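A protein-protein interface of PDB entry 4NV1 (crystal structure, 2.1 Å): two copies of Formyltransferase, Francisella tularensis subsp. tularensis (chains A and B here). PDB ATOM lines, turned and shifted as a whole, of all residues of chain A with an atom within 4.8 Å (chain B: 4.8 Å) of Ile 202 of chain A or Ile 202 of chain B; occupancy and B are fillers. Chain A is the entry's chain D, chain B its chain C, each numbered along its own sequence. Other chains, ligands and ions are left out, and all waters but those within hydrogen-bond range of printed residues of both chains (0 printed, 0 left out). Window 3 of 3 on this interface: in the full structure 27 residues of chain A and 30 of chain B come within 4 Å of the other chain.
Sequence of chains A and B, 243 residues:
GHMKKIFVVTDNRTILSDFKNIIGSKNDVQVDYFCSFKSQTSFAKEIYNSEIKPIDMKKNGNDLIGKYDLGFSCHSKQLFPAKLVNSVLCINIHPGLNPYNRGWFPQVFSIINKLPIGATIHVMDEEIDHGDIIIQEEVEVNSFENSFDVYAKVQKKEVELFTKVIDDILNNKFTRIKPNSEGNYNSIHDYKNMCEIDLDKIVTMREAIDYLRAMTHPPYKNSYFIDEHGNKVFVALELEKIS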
ATOM      1  N   ASP A 200      13.465  -2.764 -16.337  1.00  0.00           N
ATOM      2  CA  ASP A 200      14.023  -3.219 -15.057  1.00  0.00           C
ATOM      3  C   ASP A 200      13.351  -4.454 -14.488  1.00  0.00           C
ATOM      4  O   ASP A 200      13.832  -5.048 -13.540  1.00  0.00           O
ATOM      5  CB  ASP A 200      13.997  -2.021 -14.108  1.00  0.00           C
ATOM      6  CG  ASP A 200      14.889  -0.931 -14.608  1.00  0.00           C
ATOM      7  OD1 ASP A 200      16.072  -1.269 -14.868  1.00  0.00           O
ATOM      8  OD2 ASP A 200      14.423   0.212 -14.828  1.00  0.00           O
ATOM      9  N   LYS A 201      12.259  -4.903 -15.100  1.00  0.00           N
ATOM     10  CA  LYS A 201      11.581  -6.052 -14.552  1.00  0.00           C
ATOM     11  C   LYS A 201      12.394  -7.311 -14.676  1.00  0.00           C
ATOM     12  O   LYS A 201      12.991  -7.557 -15.740  1.00  0.00           O
ATOM     13  CB  LYS A 201      10.256  -6.216 -15.274  1.00  0.00           C
ATOM     14  CG  LYS A 201       9.356  -7.271 -14.709  1.00  0.00           C
ATOM     15  CD  LYS A 201       7.956  -6.981 -15.234  1.00  0.00           C
ATOM     16  CE  LYS A 201       7.300  -8.257 -15.702  1.00  0.00           C
ATOM     17  NZ  LYS A 201       7.368  -9.286 -14.638  1.00  0.00           N
ATOM     18  N   ILE A 202      12.412  -8.095 -13.596  1.00  0.00           N
ATOM     19  CA  ILE A 202      13.178  -9.334 -13.516  1.00  0.00           C
ATOM     20  C   ILE A 202      12.348 -10.486 -14.014  1.00  0.00           C
ATOM     21  O   ILE A 202      11.206 -10.554 -13.591  1.00  0.00           O
ATOM     22  CB  ILE A 202      13.471  -9.676 -12.038  1.00  0.00           C
ATOM     23  CG1 ILE A 202      14.342  -8.573 -11.424  1.00  0.00           C
ATOM     24  CG2 ILE A 202      14.047 -11.068 -11.891  1.00  0.00           C
ATOM     25  CD1 ILE A 202      15.747  -8.962 -11.016  1.00  0.00           C
ATOM     26  N   VAL A 203      12.908 -11.388 -14.837  1.00  0.00           N
ATOM     27  CA  VAL A 203      12.104 -12.399 -15.547  1.00  0.00           C
ATOM     28  C   VAL A 203      13.021 -13.570 -15.889  1.00  0.00           C
ATOM     29  O   VAL A 203      14.229 -13.432 -15.874  1.00  0.00           O
ATOM     30  CB  VAL A 203      11.450 -11.767 -16.819  1.00  0.00           C
ATOM     31  CG1 VAL A 203      10.363 -10.747 -16.466  1.00  0.00           C
ATOM     32  CG2 VAL A 203      12.471 -11.018 -17.648  1.00  0.00           C
ATOM     33  N   THR A 204      12.505 -14.756 -16.144  1.00  0.00           N
ATOM     34  CA  THR A 204      13.329 -15.787 -16.779  1.00  0.00           C
ATOM     35  C   THR A 204      13.402 -15.454 -18.287  1.00  0.00           C
ATOM     36  O   THR A 204      12.619 -14.676 -18.828  1.00  0.00           O
ATOM     37  CB  THR A 204      12.680 -17.166 -16.720  1.00  0.00           C
ATOM     38  OG1 THR A 204      11.294 -17.007 -17.052  1.00  0.00           O
ATOM     39  CG2 THR A 204      12.847 -17.851 -15.333  1.00  0.00           C
ATOM     40  N   ASP B 200      15.606 -20.966 -18.091  1.00  0.00           N
ATOM     41  CA  ASP B 200      15.435 -20.714 -16.651  1.00  0.00           C
ATOM     42  C   ASP B 200      16.249 -19.543 -16.102  1.00  0.00           C
ATOM     43  O   ASP B 200      15.941 -19.022 -15.027  1.00  0.00           O
ATOM     44  CB  ASP B 200      15.743 -21.999 -15.889  1.00  0.00           C
ATOM     45  CG  ASP B 200      14.730 -23.078 -16.217  1.00  0.00           C
ATOM     46  OD1 ASP B 200      13.530 -22.797 -16.081  1.00  0.00           O
ATOM     47  OD2 ASP B 200      15.092 -24.171 -16.676  1.00  0.00           O
ATOM     48  N   LYS B 201      17.242 -19.081 -16.860  1.00  0.00           N
ATOM     49  CA  LYS B 201      18.126 -17.995 -16.388  1.00  0.00           C
ATOM     50  C   LYS B 201      17.337 -16.777 -16.006  1.00  0.00           C
ATOM     51  O   LYS B 201      16.401 -16.404 -16.701  1.00  0.00           O
ATOM     52  CB  LYS B 201      19.093 -17.634 -17.499  1.00  0.00           C
ATOM     53  CG  LYS B 201      20.065 -16.501 -17.219  1.00  0.00           C
ATOM     54  CD  LYS B 201      21.396 -16.876 -17.829  1.00  0.00           C
ATOM     55  CE  LYS B 201      22.239 -15.663 -18.193  1.00  0.00           C
ATOM     56  NZ  LYS B 201      22.579 -14.928 -16.945  1.00  0.00           N
ATOM     57  N   ILE B 202      17.737 -16.116 -14.927  1.00  0.00           N
ATOM     58  CA  ILE B 202      17.013 -14.969 -14.393  1.00  0.00           C
ATOM     59  C   ILE B 202      17.721 -13.731 -14.904  1.00  0.00           C
ATOM     60  O   ILE B 202      18.931 -13.706 -14.892  1.00  0.00           O
ATOM     61  CB  ILE B 202      16.959 -15.044 -12.831  1.00  0.00           C
ATOM     62  CG1 ILE B 202      16.536 -16.452 -12.390  1.00  0.00           C
ATOM     63  CG2 ILE B 202      16.001 -14.033 -12.227  1.00  0.00           C
ATOM     64  CD1 ILE B 202      15.878 -16.531 -11.034  1.00  0.00           C
ATOM     65  N   VAL B 203      16.989 -12.710 -15.365  1.00  0.00           N
ATOM     66  CA  VAL B 203      17.589 -11.568 -16.077  1.00  0.00           C
ATOM     67  C   VAL B 203      16.589 -10.437 -15.972  1.00  0.00           C
ATOM     68  O   VAL B 203      15.419 -10.724 -15.694  1.00  0.00           O
ATOM     69  CB  VAL B 203      17.758 -11.836 -17.605  1.00  0.00           C
ATOM     70  CG1 VAL B 203      18.659 -13.016 -17.863  1.00  0.00           C
ATOM     71  CG2 VAL B 203      16.408 -12.097 -18.262  1.00  0.00           C
ATOM     72  N   THR B 204      16.992  -9.202 -16.250  1.00  0.00           N
ATOM     73  CA  THR B 204      16.001  -8.157 -16.463  1.00  0.00           C
ATOM     74  C   THR B 204      15.594  -8.252 -17.958  1.00  0.00           C
ATOM     75  O   THR B 204      16.289  -8.832 -18.812  1.00  0.00           O
ATOM     76  CB  THR B 204      16.611  -6.773 -16.290  1.00  0.00           C
ATOM     77  OG1 THR B 204      17.802  -6.758 -17.083  1.00  0.00           O
ATOM     78  CG2 THR B 204      16.953  -6.428 -14.808  1.00  0.00           C
ATOM     79  N   GLU B 207      18.384  -6.859 -20.094  1.00  0.00           N
ATOM     80  CA  GLU B 207      19.352  -7.890 -20.370  1.00  0.00           C
ATOM     81  C   GLU B 207      18.910  -8.925 -21.444  1.00  0.00           C
ATOM     82  O   GLU B 207      19.766  -9.452 -22.159  1.00  0.00           O
ATOM     83  CB  GLU B 207      19.607  -8.678 -19.090  1.00  0.00           C
ATOM     84  CG  GLU B 207      20.548  -8.025 -18.081  1.00  0.00           C
ATOM     85  CD  GLU B 207      20.798  -8.982 -16.913  1.00  0.00           C
ATOM     86  OE1 GLU B 207      19.843  -9.447 -16.254  1.00  0.00           O
ATOM     87  OE2 GLU B 207      21.964  -9.343 -16.656  1.00  0.00           O
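O of Val 203 of chain B is in hydrogen-bond range of N of Val 203 of chain A (2.7 Å).
Of chain B, only Ile 202 (3.6 Å) and Val 203 (3.4 Å) come within 4 Å of Ile 202 of chain A. Of the printed residues of chain B, Val 203 of chain A touches Lys 201, Ile 202 and Val 203. Of the printed residues of chain A, Lys 201 of chain B touches Val 203 (3.8 Å) and Thr 204 (3.1 Å). Of the printed residues of chain B, Lys 201 of chain A touches Val 203 (3.99 Å) and Thr 204 (3.2 Å).
CG2 of Thr 204 of chain B touches O of Asp 200 of chain A (3.6 Å). O of Val 203 of chain B touches O of Lys 201 of chain A, 3.99 Å away. Thr 204 of chain B touches Lys 201 of chain A (CA to O, 3.2 Å). CG2 of Ile 202 of chain A touches CG2 of Ile 202 of chain B (3.6 Å). Ile 202 of chain A touches Val 203 of chain B (CA to O, 3.4 Å). O of Val 203 of chain A touches O of Lys 201 of chain B, at 3.8 Å. Ile 202 of chain B touches Val 203 of chain A. Thr 204 of chain A touches Asp 200 of chain B. Lys 201 of chain B touches Thr 204 of chain A (O to CA, 3.1 Å).
Of the 5 printed residues of chain A, 5 touch a printed residue of chain B. Printed residues of chain A that touch a printed residue of chain B: Asp 200, Lys 201, Ile 202, Val 203 and Thr 204. Among the printed residues, no Asp or Glu carboxylate lies within 4 Å of a Lys or Arg side-chain nitrogen of the other chain.
The backbone NH (N) of Thr 204 of chain B is in hydrogen-bond range of the side-chain carboxylate (OE1) of Glu 207 of chain B.
Asp 200 of chain A touches Thr 204 of chain B, and with the chains exchanged Thr 204 of chain A touches Asp 200 of chain B. Lys 201 of chain A touches Thr 204 of chain B, and with the chains exchanged Thr 204 of chain A touches Lys 201 of chain B. Ile 202 of chain A touches its own counterpart, Ile 202 of chain B. Ile 202 of chain A touches Val 203 of chain B, and with the chains exchanged Val 203 of chain A touches Ile 202 of chain B. Positions printed for both chains: 200, 201, 202, 203 and 204. Of the 10 pairs that touch across the chains among the printed residues, 10 have their exchanged pair printed and touching as well.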
